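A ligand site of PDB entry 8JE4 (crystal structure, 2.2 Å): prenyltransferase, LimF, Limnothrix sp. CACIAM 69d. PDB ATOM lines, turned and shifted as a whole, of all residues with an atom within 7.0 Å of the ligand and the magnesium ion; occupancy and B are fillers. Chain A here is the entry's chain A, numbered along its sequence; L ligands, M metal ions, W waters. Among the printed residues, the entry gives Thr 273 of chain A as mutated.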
ATOM      1  N   SER A  56      22.973  20.108  20.643  1.00  0.00           N
ATOM      2  CA  SER A  56      21.774  20.929  20.615  1.00  0.00           C
ATOM      3  C   SER A  56      20.523  20.061  20.712  1.00  0.00           C
ATOM      4  O   SER A  56      20.543  18.865  20.422  1.00  0.00           O
ATOM      5  CB  SER A  56      21.705  21.773  19.339  1.00  0.00           C
ATOM      6  OG  SER A  56      20.426  22.379  19.204  1.00  0.00           O
ATOM      7  N   LYS A  58      16.259  20.525  19.672  1.00  0.00           N
ATOM      8  CA  LYS A  58      15.141  21.274  19.105  1.00  0.00           C
ATOM      9  C   LYS A  58      13.852  20.738  19.695  1.00  0.00           C
ATOM     10  O   LYS A  58      13.556  19.540  19.559  1.00  0.00           O
ATOM     11  CB  LYS A  58      15.126  21.177  17.583  1.00  0.00           C
ATOM     12  CG  LYS A  58      13.848  21.721  16.954  1.00  0.00           C
ATOM     13  CD  LYS A  58      13.841  21.544  15.449  1.00  0.00           C
ATOM     14  CE  LYS A  58      14.727  22.568  14.755  1.00  0.00           C
ATOM     15  NZ  LYS A  58      14.131  23.933  14.781  1.00  0.00           N
ATOM     16  N   LYS A  60       9.698  21.037  19.984  1.00  0.00           N
ATOM     17  CA  LYS A  60       8.439  21.492  19.392  1.00  0.00           C
ATOM     18  C   LYS A  60       7.309  20.858  20.193  1.00  0.00           C
ATOM     19  O   LYS A  60       6.971  19.693  19.984  1.00  0.00           O
ATOM     20  CB  LYS A  60       8.355  21.119  17.913  1.00  0.00           C
ATOM     21  CG  LYS A  60       9.498  21.675  17.070  1.00  0.00           C
ATOM     22  CD  LYS A  60       9.512  23.195  17.126  1.00  0.00           C
ATOM     23  CE  LYS A  60      10.857  23.742  16.682  1.00  0.00           C
ATOM     24  NZ  LYS A  60      10.930  25.211  16.911  1.00  0.00           N
ATOM     25  N   ARG A  68      21.296  16.764  16.932  1.00  0.00           N
ATOM     26  CA  ARG A  68      21.777  18.023  16.384  1.00  0.00           C
ATOM     27  C   ARG A  68      23.150  18.309  16.976  1.00  0.00           C
ATOM     28  O   ARG A  68      23.267  18.572  18.183  1.00  0.00           O
ATOM     29  CB  ARG A  68      20.806  19.162  16.710  1.00  0.00           C
ATOM     30  CG  ARG A  68      19.428  18.979  16.112  1.00  0.00           C
ATOM     31  CD  ARG A  68      18.430  19.888  16.778  1.00  0.00           C
ATOM     32  NE  ARG A  68      18.941  21.242  16.959  1.00  0.00           N
ATOM     33  CZ  ARG A  68      18.859  22.200  16.049  1.00  0.00           C
ATOM     34  NH1 ARG A  68      18.286  22.006  14.876  1.00  0.00           N
ATOM     35  NH2 ARG A  68      19.356  23.404  16.333  1.00  0.00           N
ATOM     36  N   ASP A  70      27.010  20.343  15.988  1.00  0.00           N
ATOM     37  CA  ASP A  70      27.806  21.213  15.128  1.00  0.00           C
ATOM     38  C   ASP A  70      29.243  21.239  15.625  1.00  0.00           C
ATOM     39  O   ASP A  70      29.492  21.226  16.831  1.00  0.00           O
ATOM     40  CB  ASP A  70      27.248  22.651  15.111  1.00  0.00           C
ATOM     41  CG  ASP A  70      25.820  22.711  14.609  1.00  0.00           C
ATOM     42  OD1 ASP A  70      25.527  22.100  13.563  1.00  0.00           O
ATOM     43  OD2 ASP A  70      24.979  23.371  15.268  1.00  0.00           O
ATOM     44  N   ASP A 126      21.505  17.514  11.638  1.00  0.00           N
ATOM     45  CA  ASP A 126      20.235  17.506  12.362  1.00  0.00           C
ATOM     46  C   ASP A 126      19.439  16.324  11.792  1.00  0.00           C
ATOM     47  O   ASP A 126      18.710  16.468  10.811  1.00  0.00           O
ATOM     48  CB  ASP A 126      19.482  18.824  12.212  1.00  0.00           C
ATOM     49  CG  ASP A 126      18.175  18.858  12.995  1.00  0.00           C
ATOM     50  OD1 ASP A 126      17.790  17.819  13.582  1.00  0.00           O
ATOM     51  OD2 ASP A 126      17.539  19.923  13.046  1.00  0.00           O
ATOM     52  N   ARG A 128      16.830  13.050  11.750  1.00  0.00           N
ATOM     53  CA  ARG A 128      15.521  12.605  12.202  1.00  0.00           C
ATOM     54  C   ARG A 128      15.346  11.132  11.863  1.00  0.00           C
ATOM     55  O   ARG A 128      16.138  10.534  11.122  1.00  0.00           O
ATOM     56  CB  ARG A 128      14.402  13.427  11.558  1.00  0.00           C
ATOM     57  CG  ARG A 128      14.592  14.928  11.678  1.00  0.00           C
ATOM     58  CD  ARG A 128      14.476  15.406  13.124  1.00  0.00           C
ATOM     59  NE  ARG A 128      14.888  16.798  13.269  1.00  0.00           N
ATOM     60  CZ  ARG A 128      14.110  17.843  13.015  1.00  0.00           C
ATOM     61  NH1 ARG A 128      12.873  17.692  12.591  1.00  0.00           N
ATOM     62  NH2 ARG A 128      14.602  19.069  13.190  1.00  0.00           N
ATOM     63  N   LYS A 135      18.986  16.456   7.770  1.00  0.00           N
ATOM     64  CA  LYS A 135      19.719  17.453   7.011  1.00  0.00           C
ATOM     65  C   LYS A 135      21.139  17.576   7.540  1.00  0.00           C
ATOM     66  O   LYS A 135      21.411  17.323   8.708  1.00  0.00           O
ATOM     67  CB  LYS A 135      19.001  18.807   7.047  1.00  0.00           C
ATOM     68  CG  LYS A 135      19.005  19.503   8.403  1.00  0.00           C
ATOM     69  CD  LYS A 135      18.008  20.652   8.426  1.00  0.00           C
ATOM     70  CE  LYS A 135      18.211  21.567   9.617  1.00  0.00           C
ATOM     71  NZ  LYS A 135      17.216  22.676   9.619  1.00  0.00           N
ATOM     72  N   LYS A 137      24.597  20.335   7.532  1.00  0.00           N
ATOM     73  CA  LYS A 137      24.715  21.787   7.664  1.00  0.00           C
ATOM     74  C   LYS A 137      26.153  22.239   7.465  1.00  0.00           C
ATOM     75  O   LYS A 137      27.099  21.543   7.859  1.00  0.00           O
ATOM     76  CB  LYS A 137      24.217  22.251   9.037  1.00  0.00           C
ATOM     77  CG  LYS A 137      22.881  21.645   9.439  1.00  0.00           C
ATOM     78  CD  LYS A 137      22.465  22.110  10.809  1.00  0.00           C
ATOM     79  CE  LYS A 137      22.099  23.576  10.770  1.00  0.00           C
ATOM     80  NZ  LYS A 137      20.672  23.787  10.405  1.00  0.00           N
ATOM     81  N   PHE A 139      28.326  26.087   7.835  1.00  0.00           N
ATOM     82  CA  PHE A 139      28.330  27.495   8.186  1.00  0.00           C
ATOM     83  C   PHE A 139      29.644  28.117   7.762  1.00  0.00           C
ATOM     84  O   PHE A 139      30.712  27.538   7.971  1.00  0.00           O
ATOM     85  CB  PHE A 139      28.113  27.698   9.693  1.00  0.00           C
ATOM     86  CG  PHE A 139      26.773  27.233  10.191  1.00  0.00           C
ATOM     87  CD1 PHE A 139      26.588  25.918  10.612  1.00  0.00           C
ATOM     88  CD2 PHE A 139      25.707  28.106  10.257  1.00  0.00           C
ATOM     89  CE1 PHE A 139      25.347  25.490  11.069  1.00  0.00           C
ATOM     90  CE2 PHE A 139      24.463  27.688  10.715  1.00  0.00           C
ATOM     91  CZ  PHE A 139      24.290  26.376  11.116  1.00  0.00           C
ATOM     92  N   ASP A 176      21.653  24.639   4.668  1.00  0.00           N
ATOM     93  CA  ASP A 176      20.941  23.418   5.048  1.00  0.00           C
ATOM     94  C   ASP A 176      20.843  22.510   3.826  1.00  0.00           C
ATOM     95  O   ASP A 176      20.530  22.979   2.724  1.00  0.00           O
ATOM     96  CB  ASP A 176      19.552  23.745   5.595  1.00  0.00           C
ATOM     97  CG  ASP A 176      19.573  24.082   7.068  1.00  0.00           C
ATOM     98  OD1 ASP A 176      20.666  24.079   7.664  1.00  0.00           O
ATOM     99  OD2 ASP A 176      18.483  24.319   7.647  1.00  0.00           O
ATOM    100  N   TYR A 178      18.946  19.060   3.095  1.00  0.00           N
ATOM    101  CA  TYR A 178      18.093  17.928   3.416  1.00  0.00           C
ATOM    102  C   TYR A 178      18.396  16.743   2.518  1.00  0.00           C
ATOM    103  O   TYR A 178      18.759  16.901   1.350  1.00  0.00           O
ATOM    104  CB  TYR A 178      16.617  18.318   3.295  1.00  0.00           C
ATOM    105  CG  TYR A 178      16.161  19.316   4.343  1.00  0.00           C
ATOM    106  CD1 TYR A 178      16.392  20.679   4.179  1.00  0.00           C
ATOM    107  CD2 TYR A 178      15.518  18.881   5.485  1.00  0.00           C
ATOM    108  CE1 TYR A 178      15.988  21.578   5.147  1.00  0.00           C
ATOM    109  CE2 TYR A 178      15.093  19.786   6.451  1.00  0.00           C
ATOM    110  CZ  TYR A 178      15.330  21.130   6.267  1.00  0.00           C
ATOM    111  OH  TYR A 178      14.920  22.017   7.234  1.00  0.00           O
ATOM    112  N   GLU A 186      20.652  30.644   4.906  1.00  0.00           N
ATOM    113  CA  GLU A 186      20.215  31.512   5.981  1.00  0.00           C
ATOM    114  C   GLU A 186      21.335  32.471   6.358  1.00  0.00           C
ATOM    115  O   GLU A 186      22.498  32.075   6.401  1.00  0.00           O
ATOM    116  CB  GLU A 186      19.773  30.704   7.204  1.00  0.00           C
ATOM    117  CG  GLU A 186      19.175  31.541   8.313  1.00  0.00           C
ATOM    118  CD  GLU A 186      18.496  30.706   9.375  1.00  0.00           C
ATOM    119  OE1 GLU A 186      18.731  29.476   9.403  1.00  0.00           O
ATOM    120  OE2 GLU A 186      17.736  31.270  10.187  1.00  0.00           O
ATOM    121  N   TYR A 188      22.714  35.291   9.268  1.00  0.00           N
ATOM    122  CA  TYR A 188      22.622  35.558  10.708  1.00  0.00           C
ATOM    123  C   TYR A 188      23.316  36.863  11.044  1.00  0.00           C
ATOM    124  O   TYR A 188      24.472  36.869  11.505  1.00  0.00           O
ATOM    125  CB  TYR A 188      23.225  34.415  11.525  1.00  0.00           C
ATOM    126  CG  TYR A 188      22.691  33.048  11.191  1.00  0.00           C
ATOM    127  CD1 TYR A 188      23.294  32.261  10.225  1.00  0.00           C
ATOM    128  CD2 TYR A 188      21.596  32.528  11.868  1.00  0.00           C
ATOM    129  CE1 TYR A 188      22.803  30.997   9.918  1.00  0.00           C
ATOM    130  CE2 TYR A 188      21.103  31.273  11.572  1.00  0.00           C
ATOM    131  CZ  TYR A 188      21.711  30.509  10.597  1.00  0.00           C
ATOM    132  OH  TYR A 188      21.227  29.257  10.302  1.00  0.00           O
ATOM    133  N   GLY A 226      17.936  35.206  12.521  1.00  0.00           N
ATOM    134  CA  GLY A 226      18.103  34.322  11.383  1.00  0.00           C
ATOM    135  C   GLY A 226      17.144  34.689  10.271  1.00  0.00           C
ATOM    136  O   GLY A 226      15.931  34.779  10.482  1.00  0.00           O
ATOM    137  N   SER A 228      15.927  33.632   6.445  1.00  0.00           N
ATOM    138  CA  SER A 228      15.969  32.579   5.440  1.00  0.00           C
ATOM    139  C   SER A 228      14.601  32.461   4.785  1.00  0.00           C
ATOM    140  O   SER A 228      13.592  32.665   5.470  1.00  0.00           O
ATOM    141  CB  SER A 228      16.372  31.235   6.060  1.00  0.00           C
ATOM    142  OG  SER A 228      16.251  30.191   5.112  1.00  0.00           O
ATOM    143  N   ASN A 231      12.426  29.896   6.770  1.00  0.00           N
ATOM    144  CA  ASN A 231      11.862  30.190   8.080  1.00  0.00           C
ATOM    145  C   ASN A 231      10.418  30.630   7.944  1.00  0.00           C
ATOM    146  O   ASN A 231      10.070  31.407   7.043  1.00  0.00           O
ATOM    147  CB  ASN A 231      12.677  31.292   8.779  1.00  0.00           C
ATOM    148  CG  ASN A 231      14.083  30.848   9.112  1.00  0.00           C
ATOM    149  OD1 ASN A 231      14.421  29.666   9.021  1.00  0.00           O
ATOM    150  ND2 ASN A 231      14.912  31.794   9.525  1.00  0.00           N
ATOM    151  N   VAL A 235      13.997  34.147  13.273  1.00  0.00           N
ATOM    152  CA  VAL A 235      14.386  33.488  14.514  1.00  0.00           C
ATOM    153  C   VAL A 235      15.258  34.447  15.312  1.00  0.00           C
ATOM    154  O   VAL A 235      16.126  35.123  14.742  1.00  0.00           O
ATOM    155  CB  VAL A 235      15.129  32.166  14.240  1.00  0.00           C
ATOM    156  CG1 VAL A 235      15.382  31.409  15.536  1.00  0.00           C
ATOM    157  CG2 VAL A 235      14.341  31.314  13.263  1.00  0.00           C
ATOM    158  N   TYR A 237      18.115  34.920  18.170  1.00  0.00           N
ATOM    159  CA  TYR A 237      19.230  34.180  18.747  1.00  0.00           C
ATOM    160  C   TYR A 237      19.800  34.962  19.914  1.00  0.00           C
ATOM    161  O   TYR A 237      20.101  36.156  19.789  1.00  0.00           O
ATOM    162  CB  TYR A 237      20.318  33.921  17.704  1.00  0.00           C
ATOM    163  CG  TYR A 237      20.005  32.766  16.784  1.00  0.00           C
ATOM    164  CD1 TYR A 237      19.177  32.939  15.676  1.00  0.00           C
ATOM    165  CD2 TYR A 237      20.540  31.504  17.008  1.00  0.00           C
ATOM    166  CE1 TYR A 237      18.894  31.884  14.823  1.00  0.00           C
ATOM    167  CE2 TYR A 237      20.256  30.448  16.166  1.00  0.00           C
ATOM    168  CZ  TYR A 237      19.432  30.642  15.078  1.00  0.00           C
ATOM    169  OH  TYR A 237      19.158  29.589  14.227  1.00  0.00           O
ATOM    170  N   THR A 273      23.388  29.105  23.932  1.00  0.00           N
ATOM    171  CA  THR A 273      22.624  29.809  22.922  1.00  0.00           C
ATOM    172  C   THR A 273      21.199  29.271  22.887  1.00  0.00           C
ATOM    173  O   THR A 273      20.991  28.061  22.949  1.00  0.00           O
ATOM    174  CB  THR A 273      23.268  29.681  21.525  1.00  0.00           C
ATOM    175  OG1 THR A 273      24.600  30.216  21.562  1.00  0.00           O
ATOM    176  CG2 THR A 273      22.453  30.434  20.483  1.00  0.00           C
ATOM    177  N   ALA A 275      17.518  29.774  20.643  1.00  0.00           N
ATOM    178  CA  ALA A 275      16.956  30.265  19.390  1.00  0.00           C
ATOM    179  C   ALA A 275      15.462  30.030  19.382  1.00  0.00           C
ATOM    180  O   ALA A 275      14.998  28.906  19.617  1.00  0.00           O
ATOM    181  CB  ALA A 275      17.601  29.566  18.181  1.00  0.00           C
ATOM    182  N   ASN A 290      15.233  26.220  20.126  1.00  0.00           N
ATOM    183  CA  ASN A 290      16.501  25.513  20.004  1.00  0.00           C
ATOM    184  C   ASN A 290      17.429  25.912  21.146  1.00  0.00           C
ATOM    185  O   ASN A 290      17.522  27.094  21.495  1.00  0.00           O
ATOM    186  CB  ASN A 290      17.179  25.806  18.658  1.00  0.00           C
ATOM    187  CG  ASN A 290      16.404  25.261  17.484  1.00  0.00           C
ATOM    188  OD1 ASN A 290      15.525  24.415  17.644  1.00  0.00           O
ATOM    189  ND2 ASN A 290      16.735  25.721  16.286  1.00  0.00           N
ATOM    190  N   TYR A 292      21.472  25.383  22.606  1.00  0.00           N
ATOM    191  CA  TYR A 292      22.813  25.042  22.164  1.00  0.00           C
ATOM    192  C   TYR A 292      23.773  25.097  23.344  1.00  0.00           C
ATOM    193  O   TYR A 292      23.764  26.070  24.108  1.00  0.00           O
ATOM    194  CB  TYR A 292      23.298  25.973  21.040  1.00  0.00           C
ATOM    195  CG  TYR A 292      22.387  26.024  19.828  1.00  0.00           C
ATOM    196  CD1 TYR A 292      21.262  26.832  19.816  1.00  0.00           C
ATOM    197  CD2 TYR A 292      22.674  25.284  18.687  1.00  0.00           C
ATOM    198  CE1 TYR A 292      20.442  26.893  18.714  1.00  0.00           C
ATOM    199  CE2 TYR A 292      21.856  25.336  17.574  1.00  0.00           C
ATOM    200  CZ  TYR A 292      20.729  26.143  17.591  1.00  0.00           C
ATOM    201  OH  TYR A 292      19.908  26.204  16.499  1.00  0.00           O
HETATM  202  P1  LIG L   1      17.528  25.226  12.486  1.00  0.00           P
HETATM  203  O1  LIG L   1      18.568  26.102  13.366  1.00  0.00           O
HETATM  204  P2  LIG L   1      19.985  26.780  13.014  1.00  0.00           P
HETATM  205  S1  LIG L   1      20.846  27.576  14.568  1.00  0.00           S
HETATM  206  O2  LIG L   1      18.276  23.980  12.075  1.00  0.00           O
HETATM  207  O3  LIG L   1      16.367  24.922  13.398  1.00  0.00           O
HETATM  208  O4  LIG L   1      20.726  25.639  12.396  1.00  0.00           O
HETATM  209  O5  LIG L   1      17.127  26.077  11.302  1.00  0.00           O
HETATM  210  O6  LIG L   1      19.584  27.752  11.945  1.00  0.00           O
HETATM  211 MG    MG M   1      17.936  27.853  10.723  1.00  0.00          MG
HETATM  212  O   HOH W   1      17.027  29.322  11.893  1.00  0.00           O
HETATM  213  O   HOH W   2      18.837  26.527   9.047  1.00  0.00           O
HETATM  214  O   HOH W   3      16.471  28.007   9.187  1.00  0.00           O
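OH of Tyr 292 lies close to S1 of the ligand (2.5 Å).
The side-chain amino group (NZ) of Lys 137 is in salt-bridge range of an oxygen (O4) of the ligand.
The guanidinium group (NH1) of Arg 68 lies within salt-bridge range of an oxygen (O2) of the ligand, at 3.4 Å.
An oxygen (O6) of the ligand lies close to the side-chain hydroxyl (OH) of Tyr 188, 2.8 Å away.
ND2 of Asn 290 is in hydrogen-bond range of O3 of the ligand (3.0 Å).
NZ of Lys 58 lies within salt-bridge range of O3 of the ligand, 2.8 Å away.
S1 of the ligand lies close to OH of Tyr 237 (2.6 Å).
An oxygen (O2) of the ligand is in salt-bridge range of the side-chain amino group (NZ) of Lys 135 (3.0 Å).
ND2 of Asn 290 lies close to NH2 of Arg 68.
OH of Tyr 178 is in hydrogen-bond range of NZ of Lys 135, at 3.4 Å.
The side-chain amino group (NZ) of Lys 135 lies within salt-bridge range of the side-chain carboxylate (OD2) of Asp 176 (2.9 Å).
N of Asn 290 is in hydrogen-bond range of O of Ala 275.
NH1 of Arg 68 is in salt-bridge range of OD2 of Asp 126 (2.9 Å).
The side-chain carboxylate (OE2) of Glu 186 sits at hydrogen-bond distance from the side-chain amide nitrogen (ND2) of Asn 231, 2.9 Å away.
NZ of Lys 137 lies within salt-bridge range of OD1 of Asp 176 (2.8 Å).
O of Arg 68 sits at hydrogen-bond distance from N of Ser 56, at 2.9 Å.
Phe 139 touches the ligand.
Hydrophobic or aromatic side chains that line the ligand: Phe 139, Tyr 188, Tyr 237 and Tyr 292.
Of the 23 residues printed, 10 come within 4 Å of the ligand.
Tyr 188 touches the magnesium ion (OH to MG, 3.6 Å).
The nearest printed residue that does not touch the magnesium ion is Tyr 237 (4.1 Å).
The magnesium ion is bound by O5 of the ligand, O6 of the ligand, water W1, water W3, OE1 of Glu 186 and water W2.
Water W1 lies within hydrogen-bond range of OE2 of Glu 186 (2.7 Å) and OH of Tyr 237 (3.2 Å).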
